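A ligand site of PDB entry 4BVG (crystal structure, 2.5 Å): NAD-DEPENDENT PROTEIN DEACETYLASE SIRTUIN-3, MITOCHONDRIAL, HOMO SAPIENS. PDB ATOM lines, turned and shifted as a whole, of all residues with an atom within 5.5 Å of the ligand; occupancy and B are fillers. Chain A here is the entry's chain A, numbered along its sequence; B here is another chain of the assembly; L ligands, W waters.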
ATOM      1  N   VAL A  29      20.480 -36.017 -23.985  1.00  0.00           N
ATOM      2  CA  VAL A  29      21.774 -35.662 -23.426  1.00  0.00           C
ATOM      3  C   VAL A  29      21.965 -34.179 -23.159  1.00  0.00           C
ATOM      4  O   VAL A  29      21.333 -33.315 -23.798  1.00  0.00           O
ATOM      5  CB  VAL A  29      22.976 -36.158 -24.296  1.00  0.00           C
ATOM      6  CG1 VAL A  29      22.967 -37.688 -24.430  1.00  0.00           C
ATOM      7  CG2 VAL A  29      23.023 -35.455 -25.671  1.00  0.00           C
ATOM      8  N   GLY A  30      22.856 -33.902 -22.209  1.00  0.00           N
ATOM      9  CA  GLY A  30      23.257 -32.548 -21.860  1.00  0.00           C
ATOM     10  C   GLY A  30      24.766 -32.386 -21.765  1.00  0.00           C
ATOM     11  O   GLY A  30      25.564 -33.253 -22.165  1.00  0.00           O
ATOM     12  N   ALA A  31      25.185 -31.280 -21.203  1.00  0.00           N
ATOM     13  CA  ALA A  31      26.572 -30.941 -21.234  1.00  0.00           C
ATOM     14  C   ALA A  31      27.491 -31.944 -20.430  1.00  0.00           C
ATOM     15  O   ALA A  31      28.651 -32.082 -20.726  1.00  0.00           O
ATOM     16  CB  ALA A  31      26.751 -29.485 -20.811  1.00  0.00           C
ATOM     17  N   GLY A  32      26.937 -32.671 -19.457  1.00  0.00           N
ATOM     18  CA  GLY A  32      27.686 -33.750 -18.777  1.00  0.00           C
ATOM     19  C   GLY A  32      28.370 -34.796 -19.679  1.00  0.00           C
ATOM     20  O   GLY A  32      29.362 -35.441 -19.249  1.00  0.00           O
ATOM     21  N   THR A  35      31.933 -33.027 -20.861  1.00  0.00           N
ATOM     22  CA  THR A  35      33.030 -32.729 -19.929  1.00  0.00           C
ATOM     23  C   THR A  35      34.175 -33.742 -20.048  1.00  0.00           C
ATOM     24  O   THR A  35      35.333 -33.365 -19.925  1.00  0.00           O
ATOM     25  CB  THR A  35      32.578 -32.672 -18.458  1.00  0.00           C
ATOM     26  OG1 THR A  35      31.988 -33.937 -18.126  1.00  0.00           O
ATOM     27  CG2 THR A  35      31.612 -31.540 -18.210  1.00  0.00           C
ATOM     28  N   PRO A  36      33.871 -35.032 -20.321  1.00  0.00           N
ATOM     29  CA  PRO A  36      35.037 -35.923 -20.390  1.00  0.00           C
ATOM     30  C   PRO A  36      35.911 -35.680 -21.584  1.00  0.00           C
ATOM     31  O   PRO A  36      36.983 -36.249 -21.632  1.00  0.00           O
ATOM     32  CB  PRO A  36      34.418 -37.336 -20.460  1.00  0.00           C
ATOM     33  CG  PRO A  36      33.013 -37.151 -19.947  1.00  0.00           C
ATOM     34  CD  PRO A  36      32.641 -35.795 -20.493  1.00  0.00           C
ATOM     35  N   ASP A  41      31.174 -27.852 -18.099  1.00  0.00           N
ATOM     36  CA  ASP A  41      29.738 -27.683 -18.176  1.00  0.00           C
ATOM     37  C   ASP A  41      29.163 -26.325 -17.729  1.00  0.00           C
ATOM     38  O   ASP A  41      29.820 -25.321 -17.780  1.00  0.00           O
ATOM     39  CB  ASP A  41      29.010 -28.888 -17.573  1.00  0.00           C
ATOM     40  CG  ASP A  41      29.132 -28.990 -16.083  1.00  0.00           C
ATOM     41  OD1 ASP A  41      29.439 -28.042 -15.404  1.00  0.00           O
ATOM     42  OD2 ASP A  41      28.893 -30.060 -15.563  1.00  0.00           O
ATOM     43  N   PHE A  42      27.909 -26.309 -17.316  1.00  0.00           N
ATOM     44  CA  PHE A  42      27.268 -25.059 -16.899  1.00  0.00           C
ATOM     45  C   PHE A  42      27.177 -24.854 -15.387  1.00  0.00           C
ATOM     46  O   PHE A  42      27.460 -23.746 -14.906  1.00  0.00           O
ATOM     47  CB  PHE A  42      25.880 -24.880 -17.553  1.00  0.00           C
ATOM     48  CG  PHE A  42      25.953 -24.669 -19.027  1.00  0.00           C
ATOM     49  CD1 PHE A  42      26.298 -23.392 -19.531  1.00  0.00           C
ATOM     50  CD2 PHE A  42      25.769 -25.742 -19.919  1.00  0.00           C
ATOM     51  CE1 PHE A  42      26.421 -23.182 -20.891  1.00  0.00           C
ATOM     52  CE2 PHE A  42      25.897 -25.536 -21.272  1.00  0.00           C
ATOM     53  CZ  PHE A  42      26.218 -24.260 -21.752  1.00  0.00           C
ATOM     54  N   ARG A  43      26.762 -25.928 -14.689  1.00  0.00           N
ATOM     55  CA  ARG A  43      26.279 -25.870 -13.291  1.00  0.00           C
ATOM     56  C   ARG A  43      27.105 -26.675 -12.247  1.00  0.00           C
ATOM     57  O   ARG A  43      26.730 -26.729 -11.072  1.00  0.00           O
ATOM     58  CB  ARG A  43      24.771 -26.255 -13.225  1.00  0.00           C
ATOM     59  CG  ARG A  43      23.837 -25.232 -13.857  1.00  0.00           C
ATOM     60  CD  ARG A  43      22.353 -25.622 -13.844  1.00  0.00           C
ATOM     61  NE  ARG A  43      21.598 -24.630 -14.612  1.00  0.00           N
ATOM     62  CZ  ARG A  43      21.453 -24.645 -15.954  1.00  0.00           C
ATOM     63  NH1 ARG A  43      21.976 -25.640 -16.694  1.00  0.00           N
ATOM     64  NH2 ARG A  43      20.762 -23.698 -16.564  1.00  0.00           N
ATOM     65  N   SER A  44      28.197 -27.308 -12.673  1.00  0.00           N
ATOM     66  CA  SER A  44      29.164 -27.914 -11.737  1.00  0.00           C
ATOM     67  C   SER A  44      29.897 -26.808 -10.942  1.00  0.00           C
ATOM     68  O   SER A  44      30.482 -25.914 -11.541  1.00  0.00           O
ATOM     69  CB  SER A  44      30.160 -28.821 -12.464  1.00  0.00           C
ATOM     70  OG  SER A  44      29.491 -29.969 -13.000  1.00  0.00           O
ATOM     71  N   TYR A  50      28.559 -21.376 -15.382  1.00  0.00           N
ATOM     72  CA  TYR A  50      27.729 -20.496 -14.502  1.00  0.00           C
ATOM     73  C   TYR A  50      28.302 -20.280 -13.070  1.00  0.00           C
ATOM     74  O   TYR A  50      27.597 -19.749 -12.192  1.00  0.00           O
ATOM     75  CB  TYR A  50      26.203 -20.876 -14.462  1.00  0.00           C
ATOM     76  CG  TYR A  50      25.474 -20.803 -15.809  1.00  0.00           C
ATOM     77  CD1 TYR A  50      25.997 -20.075 -16.854  1.00  0.00           C
ATOM     78  CD2 TYR A  50      24.272 -21.477 -16.020  1.00  0.00           C
ATOM     79  CE1 TYR A  50      25.374 -20.026 -18.091  1.00  0.00           C
ATOM     80  CE2 TYR A  50      23.624 -21.424 -17.255  1.00  0.00           C
ATOM     81  CZ  TYR A  50      24.183 -20.684 -18.298  1.00  0.00           C
ATOM     82  OH  TYR A  50      23.584 -20.572 -19.562  1.00  0.00           O
ATOM     83  N   PHE A  65      24.140 -16.402 -23.864  1.00  0.00           N
ATOM     84  CA  PHE A  65      23.033 -16.819 -24.734  1.00  0.00           C
ATOM     85  C   PHE A  65      21.785 -15.938 -24.589  1.00  0.00           C
ATOM     86  O   PHE A  65      20.662 -16.425 -24.719  1.00  0.00           O
ATOM     87  CB  PHE A  65      22.572 -18.236 -24.404  1.00  0.00           C
ATOM     88  CG  PHE A  65      23.639 -19.294 -24.522  1.00  0.00           C
ATOM     89  CD1 PHE A  65      24.633 -19.229 -25.527  1.00  0.00           C
ATOM     90  CD2 PHE A  65      23.601 -20.408 -23.661  1.00  0.00           C
ATOM     91  CE1 PHE A  65      25.614 -20.219 -25.623  1.00  0.00           C
ATOM     92  CE2 PHE A  65      24.582 -21.399 -23.758  1.00  0.00           C
ATOM     93  CZ  PHE A  65      25.578 -21.301 -24.745  1.00  0.00           C
ATOM     94  N   GLN A 113      21.001 -31.153 -26.047  1.00  0.00           N
ATOM     95  CA  GLN A 113      21.023 -29.762 -25.672  1.00  0.00           C
ATOM     96  C   GLN A 113      22.337 -29.093 -26.003  1.00  0.00           C
ATOM     97  O   GLN A 113      22.479 -27.877 -25.779  1.00  0.00           O
ATOM     98  CB  GLN A 113      20.823 -29.668 -24.156  1.00  0.00           C
ATOM     99  CG  GLN A 113      19.452 -30.075 -23.653  1.00  0.00           C
ATOM    100  CD  GLN A 113      19.446 -30.330 -22.138  1.00  0.00           C
ATOM    101  OE1 GLN A 113      19.195 -29.431 -21.328  1.00  0.00           O
ATOM    102  NE2 GLN A 113      19.683 -31.563 -21.767  1.00  0.00           N
ATOM    103  N   ASN A 114      23.315 -29.881 -26.486  1.00  0.00           N
ATOM    104  CA  ASN A 114      24.686 -29.385 -26.670  1.00  0.00           C
ATOM    105  C   ASN A 114      24.849 -28.697 -28.011  1.00  0.00           C
ATOM    106  O   ASN A 114      24.202 -29.062 -28.998  1.00  0.00           O
ATOM    107  CB  ASN A 114      25.705 -30.550 -26.610  1.00  0.00           C
ATOM    108  CG  ASN A 114      25.802 -31.192 -25.236  1.00  0.00           C
ATOM    109  OD1 ASN A 114      25.327 -30.617 -24.222  1.00  0.00           O
ATOM    110  ND2 ASN A 114      26.414 -32.379 -25.183  1.00  0.00           N
ATOM    111  N   ILE A 115      25.759 -27.741 -28.081  1.00  0.00           N
ATOM    112  CA  ILE A 115      26.022 -27.067 -29.342  1.00  0.00           C
ATOM    113  C   ILE A 115      27.463 -27.398 -29.820  1.00  0.00           C
ATOM    114  O   ILE A 115      27.941 -26.856 -30.837  1.00  0.00           O
ATOM    115  CB  ILE A 115      25.787 -25.530 -29.256  1.00  0.00           C
ATOM    116  CG1 ILE A 115      26.730 -24.886 -28.219  1.00  0.00           C
ATOM    117  CG2 ILE A 115      24.282 -25.229 -28.991  1.00  0.00           C
ATOM    118  CD1 ILE A 115      26.827 -23.371 -28.240  1.00  0.00           C
ATOM    119  N   HIS A 133      18.993 -27.295 -29.154  1.00  0.00           N
ATOM    120  CA  HIS A 133      19.403 -25.949 -28.737  1.00  0.00           C
ATOM    121  C   HIS A 133      20.175 -25.277 -29.867  1.00  0.00           C
ATOM    122  O   HIS A 133      20.883 -24.283 -29.646  1.00  0.00           O
ATOM    123  CB  HIS A 133      20.179 -25.951 -27.411  1.00  0.00           C
ATOM    124  CG  HIS A 133      19.317 -26.183 -26.192  1.00  0.00           C
ATOM    125  ND1 HIS A 133      19.841 -26.461 -24.949  1.00  0.00           N
ATOM    126  CD2 HIS A 133      17.963 -26.161 -26.042  1.00  0.00           C
ATOM    127  CE1 HIS A 133      18.849 -26.619 -24.089  1.00  0.00           C
ATOM    128  NE2 HIS A 133      17.706 -26.430 -24.723  1.00  0.00           N
ATOM    129  N   ILE A 176      22.266 -20.997 -33.332  1.00  0.00           N
ATOM    130  CA  ILE A 176      22.101 -21.300 -31.929  1.00  0.00           C
ATOM    131  C   ILE A 176      20.863 -20.600 -31.351  1.00  0.00           C
ATOM    132  O   ILE A 176      20.647 -19.389 -31.580  1.00  0.00           O
ATOM    133  CB  ILE A 176      23.317 -20.798 -31.116  1.00  0.00           C
ATOM    134  CG1 ILE A 176      24.627 -21.309 -31.708  1.00  0.00           C
ATOM    135  CG2 ILE A 176      23.197 -21.128 -29.624  1.00  0.00           C
ATOM    136  CD1 ILE A 176      24.813 -22.808 -31.759  1.00  0.00           C
ATOM    137  N   VAL A 177      20.083 -21.357 -30.584  1.00  0.00           N
ATOM    138  CA  VAL A 177      18.929 -20.901 -29.850  1.00  0.00           C
ATOM    139  C   VAL A 177      19.353 -20.067 -28.651  1.00  0.00           C
ATOM    140  O   VAL A 177      20.044 -20.554 -27.769  1.00  0.00           O
ATOM    141  CB  VAL A 177      18.049 -22.074 -29.353  1.00  0.00           C
ATOM    142  CG1 VAL A 177      16.733 -21.565 -28.783  1.00  0.00           C
ATOM    143  CG2 VAL A 177      17.754 -23.107 -30.456  1.00  0.00           C
ATOM    144  N   PHE A 179      18.109 -17.764 -25.211  1.00  0.00           N
ATOM    145  CA  PHE A 179      16.960 -17.706 -24.270  1.00  0.00           C
ATOM    146  C   PHE A 179      15.817 -16.863 -24.773  1.00  0.00           C
ATOM    147  O   PHE A 179      16.015 -15.777 -25.352  1.00  0.00           O
ATOM    148  CB  PHE A 179      17.393 -17.227 -22.903  1.00  0.00           C
ATOM    149  CG  PHE A 179      18.376 -18.124 -22.274  1.00  0.00           C
ATOM    150  CD1 PHE A 179      18.034 -19.426 -21.938  1.00  0.00           C
ATOM    151  CD2 PHE A 179      19.677 -17.684 -22.048  1.00  0.00           C
ATOM    152  CE1 PHE A 179      18.972 -20.290 -21.367  1.00  0.00           C
ATOM    153  CE2 PHE A 179      20.628 -18.544 -21.482  1.00  0.00           C
ATOM    154  CZ  PHE A 179      20.269 -19.846 -21.150  1.00  0.00           C
ATOM    155  N   GLY A 204      23.983 -37.153 -18.725  1.00  0.00           N
ATOM    156  CA  GLY A 204      24.754 -35.978 -18.455  1.00  0.00           C
ATOM    157  C   GLY A 204      23.977 -34.689 -18.554  1.00  0.00           C
ATOM    158  O   GLY A 204      24.418 -33.710 -19.194  1.00  0.00           O
ATOM    159  N   THR A 205      22.819 -34.674 -17.938  1.00  0.00           N
ATOM    160  CA  THR A 205      22.130 -33.408 -17.828  1.00  0.00           C
ATOM    161  C   THR A 205      21.445 -33.199 -16.466  1.00  0.00           C
ATOM    162  O   THR A 205      21.055 -34.161 -15.791  1.00  0.00           O
ATOM    163  CB  THR A 205      21.115 -33.204 -18.977  1.00  0.00           C
ATOM    164  OG1 THR A 205      20.380 -31.988 -18.721  1.00  0.00           O
ATOM    165  CG2 THR A 205      20.148 -34.334 -19.056  1.00  0.00           C
ATOM    166  N   SER A 206      21.276 -31.935 -16.093  1.00  0.00           N
ATOM    167  CA  SER A 206      20.632 -31.562 -14.819  1.00  0.00           C
ATOM    168  C   SER A 206      19.143 -31.309 -15.048  1.00  0.00           C
ATOM    169  O   SER A 206      18.401 -31.125 -14.115  1.00  0.00           O
ATOM    170  CB  SER A 206      21.250 -30.290 -14.287  1.00  0.00           C
ATOM    171  OG  SER A 206      20.911 -29.220 -15.157  1.00  0.00           O
ATOM    172  N   LEU A 207      18.753 -31.279 -16.327  1.00  0.00           N
ATOM    173  CA  LEU A 207      17.380 -31.099 -16.759  1.00  0.00           C
ATOM    174  C   LEU A 207      16.733 -29.770 -16.229  1.00  0.00           C
ATOM    175  O   LEU A 207      15.560 -29.733 -15.884  1.00  0.00           O
ATOM    176  CB  LEU A 207      16.538 -32.339 -16.410  1.00  0.00           C
ATOM    177  CG  LEU A 207      16.780 -33.710 -17.087  1.00  0.00           C
ATOM    178  CD1 LEU A 207      15.929 -34.792 -16.424  1.00  0.00           C
ATOM    179  CD2 LEU A 207      16.565 -33.787 -18.595  1.00  0.00           C
ATOM    180  N   GLU A 208      17.506 -28.695 -16.184  1.00  0.00           N
ATOM    181  CA  GLU A 208      17.042 -27.408 -15.658  1.00  0.00           C
ATOM    182  C   GLU A 208      16.620 -26.435 -16.772  1.00  0.00           C
ATOM    183  O   GLU A 208      16.434 -25.245 -16.509  1.00  0.00           O
ATOM    184  CB  GLU A 208      18.172 -26.673 -14.892  1.00  0.00           C
ATOM    185  CG  GLU A 208      18.876 -27.465 -13.803  1.00  0.00           C
ATOM    186  CD  GLU A 208      18.301 -27.201 -12.427  1.00  0.00           C
ATOM    187  OE1 GLU A 208      17.499 -26.265 -12.315  1.00  0.00           O
ATOM    188  OE2 GLU A 208      18.666 -27.933 -11.484  1.00  0.00           O
ATOM    189  N   VAL A 209      16.546 -26.894 -18.019  1.00  0.00           N
ATOM    190  CA  VAL A 209      16.116 -26.034 -19.106  1.00  0.00           C
ATOM    191  C   VAL A 209      14.906 -26.600 -19.821  1.00  0.00           C
ATOM    192  O   VAL A 209      14.799 -27.810 -20.072  1.00  0.00           O
ATOM    193  CB  VAL A 209      17.283 -25.561 -20.036  1.00  0.00           C
ATOM    194  CG1 VAL A 209      16.806 -25.287 -21.457  1.00  0.00           C
ATOM    195  CG2 VAL A 209      17.939 -24.288 -19.459  1.00  0.00           C
ATOM    196  N   ILE A 228      22.070 -41.984 -16.500  1.00  0.00           N
ATOM    197  CA  ILE A 228      23.499 -42.116 -16.182  1.00  0.00           C
ATOM    198  C   ILE A 228      24.020 -40.710 -15.990  1.00  0.00           C
ATOM    199  O   ILE A 228      24.026 -39.882 -16.915  1.00  0.00           O
ATOM    200  CB  ILE A 228      24.305 -42.829 -17.282  1.00  0.00           C
ATOM    201  CG1 ILE A 228      23.618 -44.135 -17.723  1.00  0.00           C
ATOM    202  CG2 ILE A 228      25.742 -43.036 -16.822  1.00  0.00           C
ATOM    203  CD1 ILE A 228      24.272 -44.755 -18.931  1.00  0.00           C
ATOM    204  N   ASN A 229      24.382 -40.415 -14.746  1.00  0.00           N
ATOM    205  CA  ASN A 229      24.630 -39.051 -14.351  1.00  0.00           C
ATOM    206  C   ASN A 229      25.262 -39.005 -13.011  1.00  0.00           C
ATOM    207  O   ASN A 229      25.003 -39.908 -12.230  1.00  0.00           O
ATOM    208  CB  ASN A 229      23.364 -38.220 -14.315  1.00  0.00           C
ATOM    209  CG  ASN A 229      23.655 -36.757 -14.543  1.00  0.00           C
ATOM    210  OD1 ASN A 229      24.341 -36.405 -15.525  1.00  0.00           O
ATOM    211  ND2 ASN A 229      23.227 -35.905 -13.631  1.00  0.00           N
ATOM    212  N   ARG A 230      26.083 -37.972 -12.761  1.00  0.00           N
ATOM    213  CA  ARG A 230      26.700 -37.772 -11.451  1.00  0.00           C
ATOM    214  C   ARG A 230      25.647 -37.760 -10.332  1.00  0.00           C
ATOM    215  O   ARG A 230      25.906 -38.325  -9.249  1.00  0.00           O
ATOM    216  CB  ARG A 230      27.588 -36.524 -11.426  1.00  0.00           C
ATOM    217  CG  ARG A 230      28.246 -36.151 -10.073  1.00  0.00           C
ATOM    218  CD  ARG A 230      29.399 -37.066  -9.667  1.00  0.00           C
ATOM    219  NE  ARG A 230      30.589 -36.876 -10.509  1.00  0.00           N
ATOM    220  CZ  ARG A 230      31.528 -37.790 -10.705  1.00  0.00           C
ATOM    221  NH1 ARG A 230      31.452 -38.987 -10.127  1.00  0.00           N
ATOM    222  NH2 ARG A 230      32.551 -37.505 -11.506  1.00  0.00           N
ATOM    223  N   ASP A 231      24.461 -37.190 -10.593  1.00  0.00           N
ATOM    224  CA  ASP A 231      23.398 -37.139  -9.561  1.00  0.00           C
ATOM    225  C   ASP A 231      21.965 -37.334 -10.069  1.00  0.00           C
ATOM    226  O   ASP A 231      21.678 -37.170 -11.272  1.00  0.00           O
ATOM    227  CB  ASP A 231      23.508 -35.866  -8.665  1.00  0.00           C
ATOM    228  CG  ASP A 231      24.017 -34.621  -9.425  1.00  0.00           C
ATOM    229  OD1 ASP A 231      23.528 -34.324 -10.534  1.00  0.00           O
ATOM    230  OD2 ASP A 231      24.918 -33.924  -8.881  1.00  0.00           O
ATOM    231  N   VAL A 233      18.257 -36.428 -10.855  1.00  0.00           N
ATOM    232  CA  VAL A 233      17.764 -35.119 -11.316  1.00  0.00           C
ATOM    233  C   VAL A 233      16.377 -35.238 -11.917  1.00  0.00           C
ATOM    234  O   VAL A 233      15.951 -36.338 -12.270  1.00  0.00           O
ATOM    235  CB  VAL A 233      18.684 -34.414 -12.338  1.00  0.00           C
ATOM    236  CG1 VAL A 233      19.906 -33.838 -11.649  1.00  0.00           C
ATOM    237  CG2 VAL A 233      19.118 -35.388 -13.438  1.00  0.00           C
ATOM    238  N   GLY A 249      27.256 -41.774 -10.932  1.00  0.00           N
ATOM    239  CA  GLY A 249      28.719 -41.770 -10.982  1.00  0.00           C
ATOM    240  C   GLY A 249      29.155 -41.056 -12.245  1.00  0.00           C
ATOM    241  O   GLY A 249      28.379 -40.302 -12.888  1.00  0.00           O
ATOM    242  N   ASP A 250      30.386 -41.299 -12.627  1.00  0.00           N
ATOM    243  CA  ASP A 250      30.920 -40.653 -13.777  1.00  0.00           C
ATOM    244  C   ASP A 250      30.262 -41.299 -15.025  1.00  0.00           C
ATOM    245  O   ASP A 250      30.130 -42.516 -15.115  1.00  0.00           O
ATOM    246  CB  ASP A 250      32.404 -40.830 -13.755  1.00  0.00           C
ATOM    247  CG  ASP A 250      33.013 -40.551 -15.058  1.00  0.00           C
ATOM    248  OD1 ASP A 250      33.197 -39.369 -15.358  1.00  0.00           O
ATOM    249  OD2 ASP A 250      33.275 -41.525 -15.791  1.00  0.00           O
ATOM    250  N   VAL A 251      29.865 -40.475 -15.998  1.00  0.00           N
ATOM    251  CA  VAL A 251      29.007 -40.907 -17.081  1.00  0.00           C
ATOM    252  C   VAL A 251      29.736 -41.907 -17.992  1.00  0.00           C
ATOM    253  O   VAL A 251      29.124 -42.853 -18.501  1.00  0.00           O
ATOM    254  CB  VAL A 251      28.440 -39.688 -17.899  1.00  0.00           C
ATOM    255  CG1 VAL A 251      29.554 -38.882 -18.542  1.00  0.00           C
ATOM    256  CG2 VAL A 251      27.408 -40.118 -18.941  1.00  0.00           C
ATOM    257  N   VAL A 252      31.031 -41.675 -18.203  1.00  0.00           N
ATOM    258  CA  VAL A 252      31.849 -42.606 -18.981  1.00  0.00           C
ATOM    259  C   VAL A 252      31.953 -43.991 -18.301  1.00  0.00           C
ATOM    260  O   VAL A 252      31.796 -45.027 -18.996  1.00  0.00           O
ATOM    261  CB  VAL A 252      33.223 -42.013 -19.274  1.00  0.00           C
ATOM    262  CG1 VAL A 252      34.183 -43.118 -19.783  1.00  0.00           C
ATOM    263  CG2 VAL A 252      33.063 -40.888 -20.281  1.00  0.00           C
ATOM    264  N   LYS B   5      12.980 -21.212 -25.038  1.00  0.00           N
ATOM    265  CA  LYS B   5      14.085 -21.730 -24.209  1.00  0.00           C
ATOM    266  C   LYS B   5      14.283 -20.916 -22.881  1.00  0.00           C
ATOM    267  O   LYS B   5      14.629 -19.719 -22.925  1.00  0.00           O
ATOM    268  CB  LYS B   5      15.359 -21.744 -25.075  1.00  0.00           C
ATOM    269  CG  LYS B   5      16.487 -22.536 -24.471  1.00  0.00           C
ATOM    270  CD  LYS B   5      17.764 -22.275 -25.302  1.00  0.00           C
ATOM    271  CE  LYS B   5      18.996 -22.486 -24.410  1.00  0.00           C
ATOM    272  NZ  LYS B   5      20.177 -22.428 -25.248  1.00  0.00           N
ATOM    273  N   MET B   7      15.247 -21.368 -18.300  1.00  0.00           N
ATOM    274  CA  MET B   7      15.606 -22.173 -17.131  1.00  0.00           C
ATOM    275  C   MET B   7      14.369 -22.360 -16.264  1.00  0.00           C
ATOM    276  O   MET B   7      13.538 -21.459 -16.182  1.00  0.00           O
ATOM    277  CB  MET B   7      16.738 -21.474 -16.375  1.00  0.00           C
ATOM    278  CG  MET B   7      17.904 -21.190 -17.289  1.00  0.00           C
ATOM    279  SD  MET B   7      19.275 -20.343 -16.504  1.00  0.00           S
ATOM    280  CE  MET B   7      19.680 -19.102 -17.745  1.00  0.00           C
HETATM  281  C1  LIG L   1      21.377 -23.060 -25.082  1.00  0.00           C
HETATM  282  C2  LIG L   1      22.333 -22.722 -26.236  1.00  0.00           C
HETATM  283  O1  LIG L   1      21.958 -23.741 -23.992  1.00  0.00           O
HETATM  284  C3  LIG L   1      21.422 -24.612 -22.719  1.00  0.00           C
HETATM  285  C4  LIG L   1      21.274 -23.825 -21.406  1.00  0.00           C
HETATM  286  C5  LIG L   1      21.176 -24.883 -20.278  1.00  0.00           C
HETATM  287  O2  LIG L   1      21.857 -24.365 -19.143  1.00  0.00           O
HETATM  288  O3  LIG L   1      22.396 -23.049 -21.068  1.00  0.00           O
HETATM  289  O4  LIG L   1      22.138 -25.924 -22.222  1.00  0.00           O
HETATM  290  C6  LIG L   1      21.902 -26.093 -20.754  1.00  0.00           C
HETATM  291  C7  LIG L   1      21.063 -27.294 -20.205  1.00  0.00           C
HETATM  292  O5  LIG L   1      21.733 -27.840 -19.056  1.00  0.00           O
HETATM  293  P1  LIG L   1      22.793 -29.149 -18.975  1.00  0.00           P
HETATM  294  O6  LIG L   1      23.248 -29.583 -20.441  1.00  0.00           O
HETATM  295  O7  LIG L   1      22.132 -30.245 -18.240  1.00  0.00           O
HETATM  296  O8  LIG L   1      24.104 -28.664 -18.221  1.00  0.00           O
HETATM  297  P2  LIG L   1      24.340 -28.731 -16.579  1.00  0.00           P
HETATM  298  O9  LIG L   1      25.809 -28.168 -16.431  1.00  0.00           O
HETATM  299  O10 LIG L   1      24.235 -30.269 -16.162  1.00  0.00           O
HETATM  300  C8  LIG L   1      25.397 -31.131 -16.340  1.00  0.00           C
HETATM  301  C9  LIG L   1      25.092 -32.441 -15.596  1.00  0.00           C
HETATM  302  O11 LIG L   1      25.986 -33.567 -15.867  1.00  0.00           O
HETATM  303  C10 LIG L   1      26.767 -33.855 -14.661  1.00  0.00           C
HETATM  304  N1  LIG L   1      28.209 -34.192 -15.118  1.00  0.00           N
HETATM  305  C11 LIG L   1      29.196 -33.440 -15.626  1.00  0.00           C
HETATM  306  N2  LIG L   1      30.233 -34.279 -15.904  1.00  0.00           N
HETATM  307  C12 LIG L   1      29.875 -35.545 -15.576  1.00  0.00           C
HETATM  308  C13 LIG L   1      28.623 -35.484 -15.088  1.00  0.00           C
HETATM  309  N3  LIG L   1      27.986 -36.600 -14.669  1.00  0.00           N
HETATM  310  C14 LIG L   1      28.592 -37.846 -14.724  1.00  0.00           C
HETATM  311  N4  LIG L   1      29.896 -37.858 -15.197  1.00  0.00           N
HETATM  312  C15 LIG L   1      30.494 -36.737 -15.632  1.00  0.00           C
HETATM  313  N5  LIG L   1      31.736 -36.789 -16.122  1.00  0.00           N
HETATM  314  C16 LIG L   1      26.568 -32.687 -13.720  1.00  0.00           C
HETATM  315  C17 LIG L   1      25.177 -32.153 -14.125  1.00  0.00           C
HETATM  316  O12 LIG L   1      24.103 -32.934 -13.602  1.00  0.00           O
HETATM  317  O13 LIG L   1      26.580 -33.255 -12.410  1.00  0.00           O
HETATM  318  O14 LIG L   1      23.339 -27.929 -15.809  1.00  0.00           O
HETATM  319  O   HOH W   1      23.730 -25.521 -25.022  1.00  0.00           O
HETATM  320  O   HOH W   2      24.136 -28.548 -22.698  1.00  0.00           O
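NZ of Lys 5 of chain B is bonded to C1 of the ligand (1.4 Å). An oxygen (O7) of the ligand sits at hydrogen-bond distance from the side-chain hydroxyl (OG1) of Thr 205. The backbone NH (N) of Ala 31 lies within hydrogen-bond range of an oxygen (O6) of the ligand, at 2.7 Å. The backbone NH of Val 251 is in hydrogen-bond range of a nitrogen (N4) of the ligand (2.7 Å). The backbone NH (N) of Arg 43 lies within hydrogen-bond range of an oxygen (O9) of the ligand, at 3.0 Å. O14 of the ligand is in salt-bridge range of NH1 of Arg 43. N of Ser 206 sits at hydrogen-bond distance from O7 of the ligand. OG of Ser 206 lies within hydrogen-bond range of O14 of the ligand (2.8 Å). OG1 of Thr 35 sits at hydrogen-bond distance from N2 of the ligand, at 2.9 Å. The backbone NH (N) of Phe 42 lies within hydrogen-bond range of an oxygen (O9) of the ligand (2.9 Å). N3 of the ligand is in hydrogen-bond range of N of Arg 230, 3.0 Å away. OD1 of Asp 250 is in hydrogen-bond range of N5 of the ligand. ND2 of Asn 229 lies within hydrogen-bond range of O12 of the ligand, at 3.1 Å. O3 of the ligand lies within hydrogen-bond range of OH of Tyr 50 (3.1 Å). O12 of the ligand is in hydrogen-bond range of OD1 of Asp 231.
O of Val 177 is in hydrogen-bond range of NZ of Lys 5 of chain B, 3.1 Å away. N of Thr 205 is in hydrogen-bond range of OD1 of Asn 229 (3.3 Å). The backbone NH (N) of Tyr 50 is in hydrogen-bond range of the backbone carbonyl oxygen (O) of Phe 42, at 2.7 Å. A ring nitrogen (ND1) of His 133 is in hydrogen-bond range of the backbone carbonyl oxygen (O) of Gln 113 (3.1 Å). N of Gln 113 is in hydrogen-bond range of O of Val 29, at 3.1 Å. The side-chain amide nitrogen (ND2) of Asn 229 is in hydrogen-bond range of the backbone carbonyl oxygen (O) of Asp 231, 3.1 Å away. The backbone NH of Gly 30 lies close to the backbone carbonyl oxygen of Gly 204. The backbone NH (N) of Gly 32 lies within hydrogen-bond range of the backbone carbonyl oxygen (O) of Gly 204 (2.7 Å).
Merely in contact with the ligand: Gln 113 (3.1 Å), Gly 249 (3.1 Å), Gly 30 (3.3 Å), His 133 (3.3 Å), Gly 32 (3.4 Å), Val 209 (3.4 Å), Asp 41 (3.4 Å), Val 177 (3.5 Å), Phe 65 (3.5 Å), Gly 204 (3.5 Å), Ile 176 (3.8 Å) and Phe 179 (3.8 Å). Hydrophobic or aromatic side chains within 4 Å of the ligand: Ala 31, Phe 42, Tyr 50, Phe 65, His 133, Ile 176, Phe 179, Val 209 and Val 251. Along chain A the residues within 4 Å of the ligand span positions 30 to 251. The nearest printed residue that does not touch the ligand is Leu 207 (4.02 Å).
Water W2 lies within hydrogen-bond range of O6 of the ligand (2.6 Å), OD1 of Asn 114 (2.8 Å) and N of Ala 31 (3.3 Å). Water W1 lies within hydrogen-bond range of an oxygen (O1) of the ligand (2.7 Å) and the backbone carbonyl oxygen (O) of Gln 113 (2.8 Å).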
